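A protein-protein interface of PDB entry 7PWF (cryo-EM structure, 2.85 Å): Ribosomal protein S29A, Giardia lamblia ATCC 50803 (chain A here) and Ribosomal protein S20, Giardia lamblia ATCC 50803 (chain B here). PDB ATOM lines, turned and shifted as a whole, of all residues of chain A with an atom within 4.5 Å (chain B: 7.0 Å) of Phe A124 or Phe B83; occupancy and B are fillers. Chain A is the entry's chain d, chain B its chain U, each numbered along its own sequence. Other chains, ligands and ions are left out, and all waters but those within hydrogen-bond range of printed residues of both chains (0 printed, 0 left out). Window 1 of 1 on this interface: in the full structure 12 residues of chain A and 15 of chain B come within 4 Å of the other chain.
The backbone carbonyl oxygen of Val A134 is in hydrogen-bond range of the backbone NH of Glu B84, at 3.2 Å. The side-chain amino group of Lys A125 sits at hydrogen-bond distance from the backbone carbonyl oxygen of Arg B69. NZ of Lys A135 lies within hydrogen-bond range of ND1 of His B81 (2.8 Å).
O of Leu B64 sits at hydrogen-bond distance from N of Leu B85, 2.8 Å away. NE of Arg B63 lies within salt-bridge range of OE2 of Glu B84, 2.5 Å away. The backbone NH (N) of His B81 lies within hydrogen-bond range of the backbone carbonyl oxygen (O) of Thr B68 (2.8 Å). The backbone carbonyl oxygen of Ile B66 lies within hydrogen-bond range of the backbone NH of Phe B83, at 2.9 Å. The side-chain amino group (NZ) of Lys A125 lies close to the backbone carbonyl oxygen (O) of Arg A121 (3.2 Å). The backbone carbonyl oxygen of Ala A128 sits at hydrogen-bond distance from the backbone NH of Phe A133, at 3.1 Å.
CB of Arg A121 touches OG1 of Thr B68, 3.7 Å away. Arg B69 touches Arg A121 (CB to NH2, 3.8 Å). Phe A124 touches Ile B66. CD2 of Phe B83 touches CE2 of Phe A124, 3.6 Å away. Thr B68 touches Lys A125 (OG1 to NZ, 3.8 Å). Phe A133 touches Leu B64 (CE2 to O, 3.5 Å). Phe B83 touches Phe A133 (CB to CB, 3.7 Å). Phe A133 touches Glu B84 (CA to O, 3.8 Å). Phe A133 touches Leu B85 (CE2 to CB, 3.7 Å). CG of Lys A135 touches O of Arg B82 (3.7 Å).
Printed residues of chain B within 4 Å of Phe A124: Ile B66 and Phe B83. Phe B83 touches just these residues of chain A: Phe A124, Phe A133 and Lys A135. Of the printed residues of chain B, Phe A133 touches Leu B64, Phe B83, Glu B84 and Leu B85. Printed residues of chain A within 4 Å of Arg B82: Lys A135. Printed residues of chain B within 4 Å of Val A134: Glu B84 (3.2 Å). Ile A119 touches none of the printed residues of chain B. Cys A120 touches none of the printed residues of chain B.
Hydrophobic or aromatic side chains of chain A that line the printed part of chain B: Phe A124 and Phe A133. Hydrophobic or aromatic side chains of chain B within 4 Å of the printed part of chain A: Leu B64, Ile B66, His B81, Phe B83 and Leu B85. Along chain B the printed residues that touch a printed residue of chain A span positions 64 to 85. Among the printed residues, no Asp or Glu carboxylate lies within 4 Å of a Lys or Arg side-chain nitrogen of the other chain.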
ATOM      1  N   ILE A 119      27.587  -3.690  22.791  1.00  0.00           N
ATOM      2  CA  ILE A 119      26.524  -3.448  23.755  1.00  0.00           C
ATOM      3  C   ILE A 119      25.205  -3.322  23.007  1.00  0.00           C
ATOM      4  O   ILE A 119      25.163  -2.959  21.831  1.00  0.00           O
ATOM      5  CB  ILE A 119      26.785  -2.200  24.626  1.00  0.00           C
ATOM      6  CG1 ILE A 119      27.199  -1.008  23.774  1.00  0.00           C
ATOM      7  CG2 ILE A 119      27.861  -2.471  25.638  1.00  0.00           C
ATOM      8  CD1 ILE A 119      27.564   0.195  24.601  1.00  0.00           C
ATOM      9  N   CYS A 120      24.116  -3.624  23.710  1.00  0.00           N
ATOM     10  CA  CYS A 120      22.796  -3.701  23.102  1.00  0.00           C
ATOM     11  C   CYS A 120      22.171  -2.312  22.942  1.00  0.00           C
ATOM     12  O   CYS A 120      22.655  -1.311  23.474  1.00  0.00           O
ATOM     13  CB  CYS A 120      21.882  -4.602  23.926  1.00  0.00           C
ATOM     14  SG  CYS A 120      21.064  -3.795  25.314  1.00  0.00           S
ATOM     15  N   ARG A 121      21.068  -2.267  22.191  1.00  0.00           N
ATOM     16  CA  ARG A 121      20.464  -0.993  21.820  1.00  0.00           C
ATOM     17  C   ARG A 121      19.689  -0.353  22.962  1.00  0.00           C
ATOM     18  O   ARG A 121      19.565   0.874  23.000  1.00  0.00           O
ATOM     19  CB  ARG A 121      19.571  -1.173  20.589  1.00  0.00           C
ATOM     20  CG  ARG A 121      18.253  -1.875  20.831  1.00  0.00           C
ATOM     21  CD  ARG A 121      17.380  -1.795  19.595  1.00  0.00           C
ATOM     22  NE  ARG A 121      16.019  -2.237  19.861  1.00  0.00           N
ATOM     23  CZ  ARG A 121      15.037  -1.437  20.251  1.00  0.00           C
ATOM     24  NH1 ARG A 121      13.830  -1.937  20.476  1.00  0.00           N
ATOM     25  NH2 ARG A 121      15.255  -0.141  20.399  1.00  0.00           N
ATOM     26  N   ARG A 122      19.168  -1.140  23.903  1.00  0.00           N
ATOM     27  CA  ARG A 122      18.513  -0.536  25.057  1.00  0.00           C
ATOM     28  C   ARG A 122      19.528   0.054  26.024  1.00  0.00           C
ATOM     29  O   ARG A 122      19.324   1.155  26.543  1.00  0.00           O
ATOM     30  CB  ARG A 122      17.621  -1.546  25.774  1.00  0.00           C
ATOM     31  CG  ARG A 122      16.426  -2.020  24.985  1.00  0.00           C
ATOM     32  CD  ARG A 122      16.762  -3.256  24.195  1.00  0.00           C
ATOM     33  NE  ARG A 122      15.710  -3.581  23.247  1.00  0.00           N
ATOM     34  CZ  ARG A 122      14.582  -4.193  23.579  1.00  0.00           C
ATOM     35  NH1 ARG A 122      14.360  -4.530  24.834  1.00  0.00           N
ATOM     36  NH2 ARG A 122      13.675  -4.466  22.660  1.00  0.00           N
ATOM     37  N   CYS A 123      20.633  -0.650  26.279  1.00  0.00           N
ATOM     38  CA  CYS A 123      21.653  -0.092  27.161  1.00  0.00           C
ATOM     39  C   CYS A 123      22.458   1.013  26.497  1.00  0.00           C
ATOM     40  O   CYS A 123      23.080   1.811  27.203  1.00  0.00           O
ATOM     41  CB  CYS A 123      22.603  -1.179  27.662  1.00  0.00           C
ATOM     42  SG  CYS A 123      21.822  -2.572  28.500  1.00  0.00           S
ATOM     43  N   PHE A 124      22.462   1.088  25.166  1.00  0.00           N
ATOM     44  CA  PHE A 124      23.254   2.113  24.497  1.00  0.00           C
ATOM     45  C   PHE A 124      22.639   3.495  24.655  1.00  0.00           C
ATOM     46  O   PHE A 124      23.352   4.491  24.526  1.00  0.00           O
ATOM     47  CB  PHE A 124      23.425   1.763  23.014  1.00  0.00           C
ATOM     48  CG  PHE A 124      24.311   2.716  22.254  1.00  0.00           C
ATOM     49  CD1 PHE A 124      25.675   2.485  22.165  1.00  0.00           C
ATOM     50  CD2 PHE A 124      23.787   3.829  21.617  1.00  0.00           C
ATOM     51  CE1 PHE A 124      26.499   3.351  21.471  1.00  0.00           C
ATOM     52  CE2 PHE A 124      24.608   4.703  20.924  1.00  0.00           C
ATOM     53  CZ  PHE A 124      25.961   4.462  20.850  1.00  0.00           C
ATOM     54  N   LYS A 125      21.341   3.578  24.954  1.00  0.00           N
ATOM     55  CA  LYS A 125      20.679   4.875  25.052  1.00  0.00           C
ATOM     56  C   LYS A 125      21.146   5.664  26.270  1.00  0.00           C
ATOM     57  O   LYS A 125      21.361   6.876  26.178  1.00  0.00           O
ATOM     58  CB  LYS A 125      19.159   4.698  25.094  1.00  0.00           C
ATOM     59  CG  LYS A 125      18.586   3.734  24.073  1.00  0.00           C
ATOM     60  CD  LYS A 125      17.180   3.305  24.469  1.00  0.00           C
ATOM     61  CE  LYS A 125      16.248   3.196  23.272  1.00  0.00           C
ATOM     62  NZ  LYS A 125      16.798   2.338  22.194  1.00  0.00           N
ATOM     63  N   GLU A 126      21.300   5.007  27.420  1.00  0.00           N
ATOM     64  CA  GLU A 126      21.585   5.712  28.666  1.00  0.00           C
ATOM     65  C   GLU A 126      23.059   5.737  29.040  1.00  0.00           C
ATOM     66  O   GLU A 126      23.498   6.682  29.701  1.00  0.00           O
ATOM     67  CB  GLU A 126      20.791   5.098  29.825  1.00  0.00           C
ATOM     68  CG  GLU A 126      20.928   3.594  29.958  1.00  0.00           C
ATOM     69  CD  GLU A 126      19.972   2.846  29.063  1.00  0.00           C
ATOM     70  OE1 GLU A 126      19.779   3.297  27.920  1.00  0.00           O
ATOM     71  OE2 GLU A 126      19.431   1.806  29.489  1.00  0.00           O
ATOM     72  N   ASN A 127      23.839   4.740  28.636  1.00  0.00           N
ATOM     73  CA  ASN A 127      25.276   4.790  28.854  1.00  0.00           C
ATOM     74  C   ASN A 127      26.002   5.601  27.790  1.00  0.00           C
ATOM     75  O   ASN A 127      27.219   5.769  27.890  1.00  0.00           O
ATOM     76  CB  ASN A 127      25.864   3.375  28.910  1.00  0.00           C
ATOM     77  CG  ASN A 127      25.209   2.505  29.971  1.00  0.00           C
ATOM     78  OD1 ASN A 127      24.103   2.011  29.794  1.00  0.00           O
ATOM     79  ND2 ASN A 127      25.907   2.311  31.081  1.00  0.00           N
ATOM     80  N   ALA A 128      25.289   6.106  26.779  1.00  0.00           N
ATOM     81  CA  ALA A 128      25.935   6.854  25.708  1.00  0.00           C
ATOM     82  C   ALA A 128      26.456   8.202  26.174  1.00  0.00           C
ATOM     83  O   ALA A 128      27.339   8.763  25.520  1.00  0.00           O
ATOM     84  CB  ALA A 128      24.973   7.064  24.540  1.00  0.00           C
ATOM     85  N   PHE A 133      29.133   9.448  23.128  1.00  0.00           N
ATOM     86  CA  PHE A 133      28.276   9.857  22.027  1.00  0.00           C
ATOM     87  C   PHE A 133      27.318  10.948  22.488  1.00  0.00           C
ATOM     88  O   PHE A 133      26.804  10.913  23.609  1.00  0.00           O
ATOM     89  CB  PHE A 133      27.502   8.656  21.486  1.00  0.00           C
ATOM     90  CG  PHE A 133      28.376   7.620  20.835  1.00  0.00           C
ATOM     91  CD1 PHE A 133      29.066   6.698  21.600  1.00  0.00           C
ATOM     92  CD2 PHE A 133      28.530   7.586  19.462  1.00  0.00           C
ATOM     93  CE1 PHE A 133      29.875   5.755  21.008  1.00  0.00           C
ATOM     94  CE2 PHE A 133      29.343   6.647  18.866  1.00  0.00           C
ATOM     95  CZ  PHE A 133      30.013   5.729  19.637  1.00  0.00           C
ATOM     96  N   VAL A 134      27.096  11.937  21.624  1.00  0.00           N
ATOM     97  CA  VAL A 134      26.186  13.034  21.918  1.00  0.00           C
ATOM     98  C   VAL A 134      25.409  13.382  20.654  1.00  0.00           C
ATOM     99  O   VAL A 134      25.876  13.163  19.533  1.00  0.00           O
ATOM    100  CB  VAL A 134      26.944  14.257  22.496  1.00  0.00           C
ATOM    101  CG1 VAL A 134      27.714  14.995  21.423  1.00  0.00           C
ATOM    102  CG2 VAL A 134      25.991  15.198  23.222  1.00  0.00           C
ATOM    103  N   LYS A 135      24.197  13.902  20.844  1.00  0.00           N
ATOM    104  CA  LYS A 135      23.304  14.253  19.746  1.00  0.00           C
ATOM    105  C   LYS A 135      23.583  15.669  19.258  1.00  0.00           C
ATOM    106  O   LYS A 135      23.766  16.581  20.067  1.00  0.00           O
ATOM    107  CB  LYS A 135      21.845  14.134  20.184  1.00  0.00           C
ATOM    108  CG  LYS A 135      21.400  12.721  20.507  1.00  0.00           C
ATOM    109  CD  LYS A 135      20.273  12.717  21.522  1.00  0.00           C
ATOM    110  CE  LYS A 135      19.064  13.458  20.978  1.00  0.00           C
ATOM    111  NZ  LYS A 135      18.498  12.809  19.764  1.00  0.00           N
ATOM    112  N   ARG B  63      34.039  10.394  12.168  1.00  0.00           N
ATOM    113  CA  ARG B  63      32.886  10.475  13.051  1.00  0.00           C
ATOM    114  C   ARG B  63      32.287   9.089  13.247  1.00  0.00           C
ATOM    115  O   ARG B  63      31.846   8.458  12.283  1.00  0.00           O
ATOM    116  CB  ARG B  63      31.849  11.429  12.460  1.00  0.00           C
ATOM    117  CG  ARG B  63      32.453  12.730  11.953  1.00  0.00           C
ATOM    118  CD  ARG B  63      31.459  13.575  11.171  1.00  0.00           C
ATOM    119  NE  ARG B  63      30.085  13.393  11.630  1.00  0.00           N
ATOM    120  CZ  ARG B  63      29.145  12.767  10.933  1.00  0.00           C
ATOM    121  NH1 ARG B  63      29.427  12.266   9.737  1.00  0.00           N
ATOM    122  NH2 ARG B  63      27.922  12.645  11.431  1.00  0.00           N
ATOM    123  N   LEU B  64      32.262   8.629  14.492  1.00  0.00           N
ATOM    124  CA  LEU B  64      31.580   7.395  14.845  1.00  0.00           C
ATOM    125  C   LEU B  64      30.095   7.696  15.024  1.00  0.00           C
ATOM    126  O   LEU B  64      29.721   8.463  15.913  1.00  0.00           O
ATOM    127  CB  LEU B  64      32.176   6.822  16.128  1.00  0.00           C
ATOM    128  CG  LEU B  64      33.507   6.073  16.031  1.00  0.00           C
ATOM    129  CD1 LEU B  64      34.670   7.048  16.042  1.00  0.00           C
ATOM    130  CD2 LEU B  64      33.643   5.081  17.165  1.00  0.00           C
ATOM    131  N   THR B  65      29.248   7.110  14.186  1.00  0.00           N
ATOM    132  CA  THR B  65      27.818   7.386  14.223  1.00  0.00           C
ATOM    133  C   THR B  65      27.042   6.116  14.531  1.00  0.00           C
ATOM    134  O   THR B  65      27.358   5.043  14.010  1.00  0.00           O
ATOM    135  CB  THR B  65      27.316   7.977  12.896  1.00  0.00           C
ATOM    136  OG1 THR B  65      27.098   6.927  11.952  1.00  0.00           O
ATOM    137  CG2 THR B  65      28.324   8.961  12.318  1.00  0.00           C
ATOM    138  N   ILE B  66      26.028   6.240  15.385  1.00  0.00           N
ATOM    139  CA  ILE B  66      25.088   5.155  15.647  1.00  0.00           C
ATOM    140  C   ILE B  66      23.669   5.702  15.636  1.00  0.00           C
ATOM    141  O   ILE B  66      23.362   6.663  16.345  1.00  0.00           O
ATOM    142  CB  ILE B  66      25.377   4.432  16.977  1.00  0.00           C
ATOM    143  CG1 ILE B  66      26.755   3.774  16.940  1.00  0.00           C
ATOM    144  CG2 ILE B  66      24.284   3.426  17.294  1.00  0.00           C
ATOM    145  CD1 ILE B  66      26.977   2.780  18.026  1.00  0.00           C
ATOM    146  N   THR B  67      22.802   5.072  14.855  1.00  0.00           N
ATOM    147  CA  THR B  67      21.390   5.417  14.815  1.00  0.00           C
ATOM    148  C   THR B  67      20.604   4.282  15.450  1.00  0.00           C
ATOM    149  O   THR B  67      20.781   3.118  15.077  1.00  0.00           O
ATOM    150  CB  THR B  67      20.928   5.661  13.376  1.00  0.00           C
ATOM    151  OG1 THR B  67      21.536   6.858  12.876  1.00  0.00           O
ATOM    152  CG2 THR B  67      19.423   5.819  13.318  1.00  0.00           C
ATOM    153  N   THR B  68      19.755   4.616  16.420  1.00  0.00           N
ATOM    154  CA  THR B  68      18.988   3.602  17.137  1.00  0.00           C
ATOM    155  C   THR B  68      17.591   4.124  17.445  1.00  0.00           C
ATOM    156  O   THR B  68      17.402   5.317  17.660  1.00  0.00           O
ATOM    157  CB  THR B  68      19.718   3.171  18.431  1.00  0.00           C
ATOM    158  OG1 THR B  68      18.969   2.157  19.107  1.00  0.00           O
ATOM    159  CG2 THR B  68      19.937   4.350  19.367  1.00  0.00           C
ATOM    160  N   ARG B  69      16.609   3.222  17.469  1.00  0.00           N
ATOM    161  CA  ARG B  69      15.245   3.616  17.808  1.00  0.00           C
ATOM    162  C   ARG B  69      15.183   4.219  19.209  1.00  0.00           C
ATOM    163  O   ARG B  69      15.931   3.836  20.109  1.00  0.00           O
ATOM    164  CB  ARG B  69      14.290   2.420  17.729  1.00  0.00           C
ATOM    165  CG  ARG B  69      13.900   1.999  16.322  1.00  0.00           C
ATOM    166  CD  ARG B  69      13.008   3.046  15.659  1.00  0.00           C
ATOM    167  NE  ARG B  69      11.664   3.147  16.238  1.00  0.00           N
ATOM    168  CZ  ARG B  69      10.772   2.162  16.295  1.00  0.00           C
ATOM    169  NH1 ARG B  69      11.037   0.970  15.779  1.00  0.00           N
ATOM    170  NH2 ARG B  69       9.588   2.384  16.850  1.00  0.00           N
ATOM    171  N   HIS B  81      17.060   8.077  17.298  1.00  0.00           N
ATOM    172  CA  HIS B  81      18.166   8.845  17.851  1.00  0.00           C
ATOM    173  C   HIS B  81      19.387   8.694  16.949  1.00  0.00           C
ATOM    174  O   HIS B  81      19.702   7.583  16.506  1.00  0.00           O
ATOM    175  CB  HIS B  81      18.519   8.343  19.252  1.00  0.00           C
ATOM    176  CG  HIS B  81      17.736   8.978  20.357  1.00  0.00           C
ATOM    177  ND1 HIS B  81      17.313  10.288  20.304  1.00  0.00           N
ATOM    178  CD2 HIS B  81      17.304   8.491  21.541  1.00  0.00           C
ATOM    179  CE1 HIS B  81      16.644  10.576  21.404  1.00  0.00           C
ATOM    180  NE2 HIS B  81      16.625   9.504  22.172  1.00  0.00           N
ATOM    181  N   ARG B  82      20.079   9.800  16.701  1.00  0.00           N
ATOM    182  CA  ARG B  82      21.335   9.816  15.949  1.00  0.00           C
ATOM    183  C   ARG B  82      22.453  10.275  16.884  1.00  0.00           C
ATOM    184  O   ARG B  82      22.557  11.463  17.191  1.00  0.00           O
ATOM    185  CB  ARG B  82      21.233  10.743  14.745  1.00  0.00           C
ATOM    186  CG  ARG B  82      20.258  10.298  13.679  1.00  0.00           C
ATOM    187  CD  ARG B  82      19.892  11.469  12.796  1.00  0.00           C
ATOM    188  NE  ARG B  82      18.736  12.179  13.324  1.00  0.00           N
ATOM    189  CZ  ARG B  82      17.663  12.491  12.607  1.00  0.00           C
ATOM    190  NH1 ARG B  82      17.604  12.171  11.323  1.00  0.00           N
ATOM    191  NH2 ARG B  82      16.655  13.128  13.173  1.00  0.00           N
ATOM    192  N   PHE B  83      23.289   9.340  17.330  1.00  0.00           N
ATOM    193  CA  PHE B  83      24.402   9.620  18.225  1.00  0.00           C
ATOM    194  C   PHE B  83      25.703   9.711  17.433  1.00  0.00           C
ATOM    195  O   PHE B  83      25.903   8.993  16.450  1.00  0.00           O
ATOM    196  CB  PHE B  83      24.537   8.530  19.289  1.00  0.00           C
ATOM    197  CG  PHE B  83      23.394   8.466  20.257  1.00  0.00           C
ATOM    198  CD1 PHE B  83      23.312   9.353  21.314  1.00  0.00           C
ATOM    199  CD2 PHE B  83      22.421   7.487  20.134  1.00  0.00           C
ATOM    200  CE1 PHE B  83      22.270   9.283  22.210  1.00  0.00           C
ATOM    201  CE2 PHE B  83      21.384   7.410  21.029  1.00  0.00           C
ATOM    202  CZ  PHE B  83      21.308   8.309  22.072  1.00  0.00           C
ATOM    203  N   GLU B  84      26.610  10.566  17.903  1.00  0.00           N
ATOM    204  CA  GLU B  84      27.797  10.915  17.133  1.00  0.00           C
ATOM    205  C   GLU B  84      28.967  11.219  18.059  1.00  0.00           C
ATOM    206  O   GLU B  84      28.842  12.030  18.981  1.00  0.00           O
ATOM    207  CB  GLU B  84      27.498  12.106  16.218  1.00  0.00           C
ATOM    208  CG  GLU B  84      28.683  12.705  15.512  1.00  0.00           C
ATOM    209  CD  GLU B  84      28.309  13.957  14.741  1.00  0.00           C
ATOM    210  OE1 GLU B  84      27.503  14.755  15.256  1.00  0.00           O
ATOM    211  OE2 GLU B  84      28.804  14.134  13.609  1.00  0.00           O
ATOM    212  N   LEU B  85      30.093  10.558  17.805  1.00  0.00           N
ATOM    213  CA  LEU B  85      31.357  10.734  18.517  1.00  0.00           C
ATOM    214  C   LEU B  85      32.414  11.189  17.521  1.00  0.00           C
ATOM    215  O   LEU B  85      32.828  10.416  16.655  1.00  0.00           O
ATOM    216  CB  LEU B  85      31.783   9.437  19.201  1.00  0.00           C
ATOM    217  CG  LEU B  85      32.943   9.487  20.196  1.00  0.00           C
ATOM    218  CD1 LEU B  85      32.510   9.919  21.558  1.00  0.00           C
ATOM    219  CD2 LEU B  85      33.585   8.116  20.273  1.00  0.00           C
